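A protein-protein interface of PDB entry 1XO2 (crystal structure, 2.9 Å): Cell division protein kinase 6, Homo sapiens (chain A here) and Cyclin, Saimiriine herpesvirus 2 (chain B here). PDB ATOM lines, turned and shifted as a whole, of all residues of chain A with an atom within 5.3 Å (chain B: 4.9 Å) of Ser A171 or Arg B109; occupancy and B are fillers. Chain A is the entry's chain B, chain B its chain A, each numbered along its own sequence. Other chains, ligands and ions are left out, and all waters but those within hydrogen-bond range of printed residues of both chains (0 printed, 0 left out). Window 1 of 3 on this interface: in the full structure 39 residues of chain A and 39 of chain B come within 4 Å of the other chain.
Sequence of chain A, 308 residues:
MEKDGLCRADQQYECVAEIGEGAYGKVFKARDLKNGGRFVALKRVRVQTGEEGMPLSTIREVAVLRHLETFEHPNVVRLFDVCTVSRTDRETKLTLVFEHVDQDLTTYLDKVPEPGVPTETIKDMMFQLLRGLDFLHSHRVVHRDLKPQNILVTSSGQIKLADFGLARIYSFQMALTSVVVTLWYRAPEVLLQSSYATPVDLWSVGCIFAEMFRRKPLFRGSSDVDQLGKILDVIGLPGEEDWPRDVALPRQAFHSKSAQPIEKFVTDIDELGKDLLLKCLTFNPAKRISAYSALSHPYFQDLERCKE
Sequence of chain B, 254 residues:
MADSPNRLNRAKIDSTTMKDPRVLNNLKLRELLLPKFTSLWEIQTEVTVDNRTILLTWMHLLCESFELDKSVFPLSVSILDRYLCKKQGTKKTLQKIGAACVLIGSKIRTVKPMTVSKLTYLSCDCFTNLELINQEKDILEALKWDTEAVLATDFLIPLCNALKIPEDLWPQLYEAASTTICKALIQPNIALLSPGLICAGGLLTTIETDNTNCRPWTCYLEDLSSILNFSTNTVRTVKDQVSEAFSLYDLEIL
Arg A140 touches Met B18.
Arg A168 touches Arg B109 (NH2 to O, 3.9 Å).
Arg A168 touches Val B111 (NH2 to N, 3.6 Å).
Ile A169 touches Arg B109 (CG2 to NH2, 3.6 Å).
CG1 of Ile A169 touches OE2 of Glu B148, at 3.5 Å.
OH of Tyr A170 touches CB of Lys B12 (2.9 Å).
OG of Ser B71 touches OG of Ser A171, at 3.9 Å.
NH1 of Arg B109 touches OG of Ser A171 (3.7 Å).
O of Phe A172 touches OH of Tyr B174 (3.6 Å).
NE2 of Gln A173 touches CD2 of Tyr B174, 3.4 Å away.
Printed residues of chain B that touch a printed residue of chain A: Lys B12, Met B18, Asp B69, Ser B71, Arg B109, Thr B110, Val B111, Glu B148, Asp B154 and Tyr B174.
Of the 8 printed residues of chain A, 8 touch a printed residue of chain B.
Hydrophobic or aromatic side chains of chain A within 4 Å of the printed part of chain B: Ile A169, Tyr A170 and Phe A172.
Among the printed residues, Asp or Glu carboxylates within 4 Å of a Lys or Arg side-chain nitrogen of the other chain: Arg A140 with Asp B154.
Of chain B, only Ser B71 and Arg B109 come within 4 Å of Ser A171.
Arg B109 touches three residues of chain A.
Printed residues of chain A within 4 Å of Asp B154: Arg A140.
Of the printed residues of chain A, Lys B12 touches Tyr A170, Gln A173 and Met A174.
The nearest residue of chain B that does not touch Ser A171 is Lys B12 (4.3 Å).
The nearest residue of chain A that does not touch Arg B109 is Met A174 (4.4 Å).
The nearest printed residue of chain A that does not touch Val B111 is Met A174 (6.4 Å).
N of Lys B12 lies within hydrogen-bond range of O of Met A174.
SD of Met B18 sits close to O of Tyr A170, at 3.2 Å.
OD1 of Asp B154 lies within salt-bridge range of NH2 of Arg A140 (3.2 Å).
The backbone NH (N) of Gln A173 is in hydrogen-bond range of the backbone carbonyl oxygen (O) of Lys B12.
NH2 of Arg B109 lies within salt-bridge range of OE1 of Glu B148 (2.8 Å).
The side-chain sulfur (SD) of Met A174 lies within hydrogen-bond range of the backbone NH (N) of Ser A171, at 3.6 Å.
The side-chain carboxylate (OD1) of Asp B69 sits at hydrogen-bond distance from the side-chain hydroxyl (OG1) of Thr B110.
OG of Ser B71 lies close to NH1 of Arg B109 (3.1 Å).
OG of Ser A171 sits at hydrogen-bond distance from NH2 of Arg A140.
The side-chain carboxylate (OD2) of Asp B154 sits at hydrogen-bond distance from the backbone NH (N) of Leu B151, at 3.0 Å.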
ATOM      1  N   ARG A 140     -22.539  25.682  -3.084  1.00  0.00           N
ATOM      2  CA  ARG A 140     -23.026  26.658  -4.052  1.00  0.00           C
ATOM      3  C   ARG A 140     -24.512  26.536  -4.439  1.00  0.00           C
ATOM      4  O   ARG A 140     -24.906  26.917  -5.546  1.00  0.00           O
ATOM      5  CB  ARG A 140     -22.148  26.604  -5.305  1.00  0.00           C
ATOM      6  CG  ARG A 140     -20.705  27.065  -5.091  1.00  0.00           C
ATOM      7  CD  ARG A 140     -19.781  26.587  -6.234  1.00  0.00           C
ATOM      8  NE  ARG A 140     -20.508  26.405  -7.489  1.00  0.00           N
ATOM      9  CZ  ARG A 140     -20.463  27.244  -8.518  1.00  0.00           C
ATOM     10  NH1 ARG A 140     -19.715  28.331  -8.463  1.00  0.00           N
ATOM     11  NH2 ARG A 140     -21.192  27.005  -9.594  1.00  0.00           N
ATOM     12  N   ARG A 168     -31.267  26.032  -7.043  1.00  0.00           N
ATOM     13  CA  ARG A 168     -30.379  25.964  -8.197  1.00  0.00           C
ATOM     14  C   ARG A 168     -28.924  26.264  -7.858  1.00  0.00           C
ATOM     15  O   ARG A 168     -28.633  26.988  -6.906  1.00  0.00           O
ATOM     16  CB  ARG A 168     -30.870  26.886  -9.324  1.00  0.00           C
ATOM     17  CG  ARG A 168     -30.994  28.341  -8.982  1.00  0.00           C
ATOM     18  CD  ARG A 168     -31.758  29.117 -10.064  1.00  0.00           C
ATOM     19  NE  ARG A 168     -31.080  29.196 -11.361  1.00  0.00           N
ATOM     20  CZ  ARG A 168     -31.302  30.166 -12.254  1.00  0.00           C
ATOM     21  NH1 ARG A 168     -32.182  31.141 -11.988  1.00  0.00           N
ATOM     22  NH2 ARG A 168     -30.643  30.170 -13.411  1.00  0.00           N
ATOM     23  N   ILE A 169     -28.019  25.657  -8.624  1.00  0.00           N
ATOM     24  CA  ILE A 169     -26.579  25.838  -8.455  1.00  0.00           C
ATOM     25  C   ILE A 169     -26.264  27.278  -8.873  1.00  0.00           C
ATOM     26  O   ILE A 169     -26.396  27.638 -10.041  1.00  0.00           O
ATOM     27  CB  ILE A 169     -25.807  24.850  -9.360  1.00  0.00           C
ATOM     28  CG1 ILE A 169     -26.132  23.411  -8.963  1.00  0.00           C
ATOM     29  CG2 ILE A 169     -24.325  25.105  -9.273  1.00  0.00           C
ATOM     30  CD1 ILE A 169     -25.391  22.903  -7.754  1.00  0.00           C
ATOM     31  N   TYR A 170     -25.845  28.083  -7.901  1.00  0.00           N
ATOM     32  CA  TYR A 170     -25.540  29.505  -8.071  1.00  0.00           C
ATOM     33  C   TYR A 170     -24.122  29.804  -8.559  1.00  0.00           C
ATOM     34  O   TYR A 170     -23.153  29.550  -7.859  1.00  0.00           O
ATOM     35  CB  TYR A 170     -25.788  30.207  -6.732  1.00  0.00           C
ATOM     36  CG  TYR A 170     -25.663  31.706  -6.767  1.00  0.00           C
ATOM     37  CD1 TYR A 170     -26.670  32.504  -7.325  1.00  0.00           C
ATOM     38  CD2 TYR A 170     -24.528  32.333  -6.252  1.00  0.00           C
ATOM     39  CE1 TYR A 170     -26.541  33.887  -7.367  1.00  0.00           C
ATOM     40  CE2 TYR A 170     -24.387  33.710  -6.287  1.00  0.00           C
ATOM     41  CZ  TYR A 170     -25.394  34.482  -6.846  1.00  0.00           C
ATOM     42  OH  TYR A 170     -25.237  35.846  -6.886  1.00  0.00           O
ATOM     43  N   SER A 171     -24.012  30.370  -9.758  1.00  0.00           N
ATOM     44  CA  SER A 171     -22.711  30.698 -10.334  1.00  0.00           C
ATOM     45  C   SER A 171     -22.648  32.169 -10.740  1.00  0.00           C
ATOM     46  O   SER A 171     -23.658  32.768 -11.067  1.00  0.00           O
ATOM     47  CB  SER A 171     -22.420  29.816 -11.562  1.00  0.00           C
ATOM     48  OG  SER A 171     -23.009  28.533 -11.439  1.00  0.00           O
ATOM     49  N   PHE A 172     -21.441  32.726 -10.714  1.00  0.00           N
ATOM     50  CA  PHE A 172     -21.172  34.115 -11.068  1.00  0.00           C
ATOM     51  C   PHE A 172     -21.757  34.519 -12.427  1.00  0.00           C
ATOM     52  O   PHE A 172     -21.754  33.735 -13.394  1.00  0.00           O
ATOM     53  CB  PHE A 172     -19.653  34.356 -11.085  1.00  0.00           C
ATOM     54  CG  PHE A 172     -19.258  35.807 -11.020  1.00  0.00           C
ATOM     55  CD1 PHE A 172     -19.627  36.587  -9.931  1.00  0.00           C
ATOM     56  CD2 PHE A 172     -18.483  36.389 -12.030  1.00  0.00           C
ATOM     57  CE1 PHE A 172     -19.233  37.926  -9.836  1.00  0.00           C
ATOM     58  CE2 PHE A 172     -18.077  37.739 -11.942  1.00  0.00           C
ATOM     59  CZ  PHE A 172     -18.456  38.502 -10.840  1.00  0.00           C
ATOM     60  N   GLN A 173     -22.240  35.765 -12.467  1.00  0.00           N
ATOM     61  CA  GLN A 173     -22.838  36.396 -13.647  1.00  0.00           C
ATOM     62  C   GLN A 173     -23.999  35.644 -14.260  1.00  0.00           C
ATOM     63  O   GLN A 173     -24.337  35.860 -15.418  1.00  0.00           O
ATOM     64  CB  GLN A 173     -21.773  36.671 -14.719  1.00  0.00           C
ATOM     65  CG  GLN A 173     -20.880  37.869 -14.409  1.00  0.00           C
ATOM     66  CD  GLN A 173     -19.812  38.104 -15.472  1.00  0.00           C
ATOM     67  OE1 GLN A 173     -19.112  39.121 -15.446  1.00  0.00           O
ATOM     68  NE2 GLN A 173     -19.676  37.160 -16.411  1.00  0.00           N
ATOM     69  N   MET A 174     -24.604  34.763 -13.470  1.00  0.00           N
ATOM     70  CA  MET A 174     -25.755  33.965 -13.907  1.00  0.00           C
ATOM     71  C   MET A 174     -26.995  34.865 -13.878  1.00  0.00           C
ATOM     72  O   MET A 174     -27.167  35.656 -12.948  1.00  0.00           O
ATOM     73  CB  MET A 174     -25.913  32.756 -12.969  1.00  0.00           C
ATOM     74  CG  MET A 174     -27.324  32.431 -12.484  1.00  0.00           C
ATOM     75  SD  MET A 174     -27.262  31.417 -10.949  1.00  0.00           S
ATOM     76  CE  MET A 174     -27.935  29.849 -11.515  1.00  0.00           C
ATOM     77  N   LYS B  12     -26.379  37.649 -11.484  1.00  0.00           N
ATOM     78  CA  LYS B  12     -25.843  37.539 -10.124  1.00  0.00           C
ATOM     79  C   LYS B  12     -24.431  38.060  -9.879  1.00  0.00           C
ATOM     80  O   LYS B  12     -23.545  37.869 -10.706  1.00  0.00           O
ATOM     81  CB  LYS B  12     -25.935  36.097  -9.665  1.00  0.00           C
ATOM     82  N   MET B  18     -20.726  32.020  -0.859  1.00  0.00           N
ATOM     83  CA  MET B  18     -20.850  31.049  -1.934  1.00  0.00           C
ATOM     84  C   MET B  18     -19.512  30.915  -2.664  1.00  0.00           C
ATOM     85  O   MET B  18     -19.220  29.881  -3.275  1.00  0.00           O
ATOM     86  CB  MET B  18     -21.943  31.486  -2.900  1.00  0.00           C
ATOM     87  CG  MET B  18     -22.119  30.581  -4.081  1.00  0.00           C
ATOM     88  SD  MET B  18     -21.733  31.433  -5.652  1.00  0.00           S
ATOM     89  CE  MET B  18     -20.049  30.715  -6.043  1.00  0.00           C
ATOM     90  N   ASP B  69     -26.694  30.886 -20.239  1.00  0.00           N
ATOM     91  CA  ASP B  69     -25.708  31.053 -19.174  1.00  0.00           C
ATOM     92  C   ASP B  69     -24.515  30.123 -19.438  1.00  0.00           C
ATOM     93  O   ASP B  69     -24.675  28.963 -19.808  1.00  0.00           O
ATOM     94  CB  ASP B  69     -26.342  30.753 -17.802  1.00  0.00           C
ATOM     95  CG  ASP B  69     -27.094  31.969 -17.199  1.00  0.00           C
ATOM     96  OD1 ASP B  69     -28.180  31.775 -16.593  1.00  0.00           O
ATOM     97  OD2 ASP B  69     -26.597  33.114 -17.313  1.00  0.00           O
ATOM     98  N   SER B  71     -22.870  28.132 -18.000  1.00  0.00           N
ATOM     99  CA  SER B  71     -22.873  26.780 -17.443  1.00  0.00           C
ATOM    100  C   SER B  71     -23.669  25.720 -18.208  1.00  0.00           C
ATOM    101  O   SER B  71     -23.554  24.519 -17.910  1.00  0.00           O
ATOM    102  CB  SER B  71     -23.368  26.821 -15.997  1.00  0.00           C
ATOM    103  OG  SER B  71     -22.461  27.519 -15.154  1.00  0.00           O
ATOM    104  N   VAL B  72     -24.478  26.161 -19.177  1.00  0.00           N
ATOM    105  CA  VAL B  72     -25.316  25.266 -19.979  1.00  0.00           C
ATOM    106  C   VAL B  72     -24.518  24.268 -20.828  1.00  0.00           C
ATOM    107  O   VAL B  72     -24.638  23.049 -20.669  1.00  0.00           O
ATOM    108  CB  VAL B  72     -26.260  26.088 -20.898  1.00  0.00           C
ATOM    109  CG1 VAL B  72     -27.101  25.159 -21.789  1.00  0.00           C
ATOM    110  CG2 VAL B  72     -27.178  26.947 -20.044  1.00  0.00           C
ATOM    111  N   LEU B  75     -22.683  21.459 -19.148  1.00  0.00           N
ATOM    112  CA  LEU B  75     -23.529  20.552 -18.377  1.00  0.00           C
ATOM    113  C   LEU B  75     -24.161  19.637 -19.418  1.00  0.00           C
ATOM    114  O   LEU B  75     -24.457  18.454 -19.162  1.00  0.00           O
ATOM    115  CB  LEU B  75     -24.620  21.319 -17.620  1.00  0.00           C
ATOM    116  CG  LEU B  75     -25.240  20.672 -16.368  1.00  0.00           C
ATOM    117  CD1 LEU B  75     -26.738  20.868 -16.382  1.00  0.00           C
ATOM    118  CD2 LEU B  75     -24.900  19.188 -16.295  1.00  0.00           C
ATOM    119  N   GLY B 105     -29.977  20.354 -19.941  1.00  0.00           N
ATOM    120  CA  GLY B 105     -28.950  21.206 -19.365  1.00  0.00           C
ATOM    121  C   GLY B 105     -29.378  22.638 -19.153  1.00  0.00           C
ATOM    122  O   GLY B 105     -29.149  23.199 -18.087  1.00  0.00           O
ATOM    123  N   SER B 106     -30.003  23.219 -20.176  1.00  0.00           N
ATOM    124  CA  SER B 106     -30.478  24.606 -20.140  1.00  0.00           C
ATOM    125  C   SER B 106     -31.614  24.822 -19.140  1.00  0.00           C
ATOM    126  O   SER B 106     -31.674  25.856 -18.488  1.00  0.00           O
ATOM    127  CB  SER B 106     -30.934  25.032 -21.527  1.00  0.00           C
ATOM    128  OG  SER B 106     -32.017  24.233 -21.956  1.00  0.00           O
ATOM    129  N   LYS B 107     -32.513  23.849 -19.028  1.00  0.00           N
ATOM    130  CA  LYS B 107     -33.619  23.927 -18.079  1.00  0.00           C
ATOM    131  C   LYS B 107     -33.087  24.190 -16.658  1.00  0.00           C
ATOM    132  O   LYS B 107     -33.671  24.965 -15.887  1.00  0.00           O
ATOM    133  CB  LYS B 107     -34.411  22.614 -18.089  1.00  0.00           C
ATOM    134  CG  LYS B 107     -35.234  22.419 -19.340  1.00  0.00           C
ATOM    135  CD  LYS B 107     -36.113  21.186 -19.240  1.00  0.00           C
ATOM    136  CE  LYS B 107     -37.219  21.228 -20.282  1.00  0.00           C
ATOM    137  NZ  LYS B 107     -38.077  20.014 -20.290  1.00  0.00           N
ATOM    138  N   ILE B 108     -31.962  23.556 -16.341  1.00  0.00           N
ATOM    139  CA  ILE B 108     -31.329  23.665 -15.041  1.00  0.00           C
ATOM    140  C   ILE B 108     -30.475  24.911 -14.794  1.00  0.00           C
ATOM    141  O   ILE B 108     -30.800  25.742 -13.934  1.00  0.00           O
ATOM    142  CB  ILE B 108     -30.435  22.442 -14.805  1.00  0.00           C
ATOM    143  CG1 ILE B 108     -31.292  21.183 -14.751  1.00  0.00           C
ATOM    144  CG2 ILE B 108     -29.608  22.621 -13.542  1.00  0.00           C
ATOM    145  CD1 ILE B 108     -30.501  19.931 -14.969  1.00  0.00           C
ATOM    146  N   ARG B 109     -29.386  25.039 -15.549  1.00  0.00           N
ATOM    147  CA  ARG B 109     -28.456  26.147 -15.354  1.00  0.00           C
ATOM    148  C   ARG B 109     -28.738  27.550 -15.910  1.00  0.00           C
ATOM    149  O   ARG B 109     -27.915  28.461 -15.682  1.00  0.00           O
ATOM    150  CB  ARG B 109     -27.062  25.721 -15.805  1.00  0.00           C
ATOM    151  CG  ARG B 109     -26.494  24.530 -15.064  1.00  0.00           C
ATOM    152  CD  ARG B 109     -26.447  24.740 -13.559  1.00  0.00           C
ATOM    153  NE  ARG B 109     -25.457  23.868 -12.933  1.00  0.00           N
ATOM    154  CZ  ARG B 109     -24.173  24.192 -12.811  1.00  0.00           C
ATOM    155  NH1 ARG B 109     -23.741  25.370 -13.264  1.00  0.00           N
ATOM    156  NH2 ARG B 109     -23.313  23.336 -12.261  1.00  0.00           N
ATOM    157  N   THR B 110     -29.851  27.749 -16.626  1.00  0.00           N
ATOM    158  CA  THR B 110     -30.160  29.085 -17.144  1.00  0.00           C
ATOM    159  C   THR B 110     -31.627  29.472 -16.922  1.00  0.00           C
ATOM    160  O   THR B 110     -32.528  28.634 -16.939  1.00  0.00           O
ATOM    161  CB  THR B 110     -29.807  29.219 -18.650  1.00  0.00           C
ATOM    162  OG1 THR B 110     -29.600  30.602 -18.973  1.00  0.00           O
ATOM    163  CG2 THR B 110     -30.933  28.687 -19.517  1.00  0.00           C
ATOM    164  N   VAL B 111     -31.859  30.761 -16.726  1.00  0.00           N
ATOM    165  CA  VAL B 111     -33.199  31.257 -16.467  1.00  0.00           C
ATOM    166  C   VAL B 111     -34.220  31.051 -17.592  1.00  0.00           C
ATOM    167  O   VAL B 111     -35.316  30.546 -17.341  1.00  0.00           O
ATOM    168  CB  VAL B 111     -33.150  32.745 -16.064  1.00  0.00           C
ATOM    169  CG1 VAL B 111     -32.594  33.571 -17.188  1.00  0.00           C
ATOM    170  CG2 VAL B 111     -34.530  33.211 -15.662  1.00  0.00           C
ATOM    171  N   GLU B 148     -27.559  16.876 -12.630  1.00  0.00           N
ATOM    172  CA  GLU B 148     -26.507  17.822 -12.257  1.00  0.00           C
ATOM    173  C   GLU B 148     -25.078  17.229 -12.213  1.00  0.00           C
ATOM    174  O   GLU B 148     -24.888  16.010 -12.331  1.00  0.00           O
ATOM    175  CB  GLU B 148     -26.864  18.443 -10.911  1.00  0.00           C
ATOM    176  CG  GLU B 148     -25.991  19.614 -10.514  1.00  0.00           C
ATOM    177  CD  GLU B 148     -26.132  20.810 -11.449  1.00  0.00           C
ATOM    178  OE1 GLU B 148     -25.126  21.196 -12.085  1.00  0.00           O
ATOM    179  OE2 GLU B 148     -27.242  21.374 -11.544  1.00  0.00           O
ATOM    180  N   ALA B 149     -24.079  18.103 -12.065  1.00  0.00           N
ATOM    181  CA  ALA B 149     -22.678  17.673 -12.016  1.00  0.00           C
ATOM    182  C   ALA B 149     -21.705  18.833 -11.772  1.00  0.00           C
ATOM    183  O   ALA B 149     -22.103  20.007 -11.835  1.00  0.00           O
ATOM    184  CB  ALA B 149     -22.310  16.964 -13.309  1.00  0.00           C
ATOM    185  N   LEU B 151     -18.976  21.196 -12.922  1.00  0.00           N
ATOM    186  CA  LEU B 151     -18.537  21.713 -14.214  1.00  0.00           C
ATOM    187  C   LEU B 151     -17.206  22.432 -14.181  1.00  0.00           C
ATOM    188  O   LEU B 151     -16.908  23.152 -13.233  1.00  0.00           O
ATOM    189  CB  LEU B 151     -19.587  22.656 -14.769  1.00  0.00           C
ATOM    190  CG  LEU B 151     -20.956  22.000 -14.842  1.00  0.00           C
ATOM    191  CD1 LEU B 151     -21.890  22.857 -15.698  1.00  0.00           C
ATOM    192  CD2 LEU B 151     -20.805  20.590 -15.428  1.00  0.00           C
ATOM    193  N   ASP B 154     -17.380  25.645 -13.090  1.00  0.00           N
ATOM    194  CA  ASP B 154     -17.669  25.944 -11.689  1.00  0.00           C
ATOM    195  C   ASP B 154     -16.457  26.505 -10.902  1.00  0.00           C
ATOM    196  O   ASP B 154     -16.641  27.296  -9.973  1.00  0.00           O
ATOM    197  CB  ASP B 154     -18.201  24.688 -10.949  1.00  0.00           C
ATOM    198  CG  ASP B 154     -19.654  24.311 -11.323  1.00  0.00           C
ATOM    199  OD1 ASP B 154     -20.360  25.112 -11.989  1.00  0.00           O
ATOM    200  OD2 ASP B 154     -20.090  23.196 -10.926  1.00  0.00           O
ATOM    201  N   TYR B 174     -13.505  36.355 -15.691  1.00  0.00           N
ATOM    202  CA  TYR B 174     -14.512  35.294 -15.771  1.00  0.00           C
ATOM    203  C   TYR B 174     -15.094  35.199 -17.175  1.00  0.00           C
ATOM    204  O   TYR B 174     -15.239  34.104 -17.731  1.00  0.00           O
ATOM    205  CB  TYR B 174     -15.672  35.560 -14.802  1.00  0.00           C
ATOM    206  CG  TYR B 174     -16.717  34.458 -14.778  1.00  0.00           C
ATOM    207  CD1 TYR B 174     -16.643  33.415 -13.845  1.00  0.00           C
ATOM    208  CD2 TYR B 174     -17.750  34.427 -15.726  1.00  0.00           C
ATOM    209  CE1 TYR B 174     -17.559  32.376 -13.858  1.00  0.00           C
ATOM    210  CE2 TYR B 174     -18.684  33.385 -15.752  1.00  0.00           C
ATOM    211  CZ  TYR B 174     -18.582  32.361 -14.816  1.00  0.00           C
ATOM    212  OH  TYR B 174     -19.491  31.318 -14.832  1.00  0.00           O
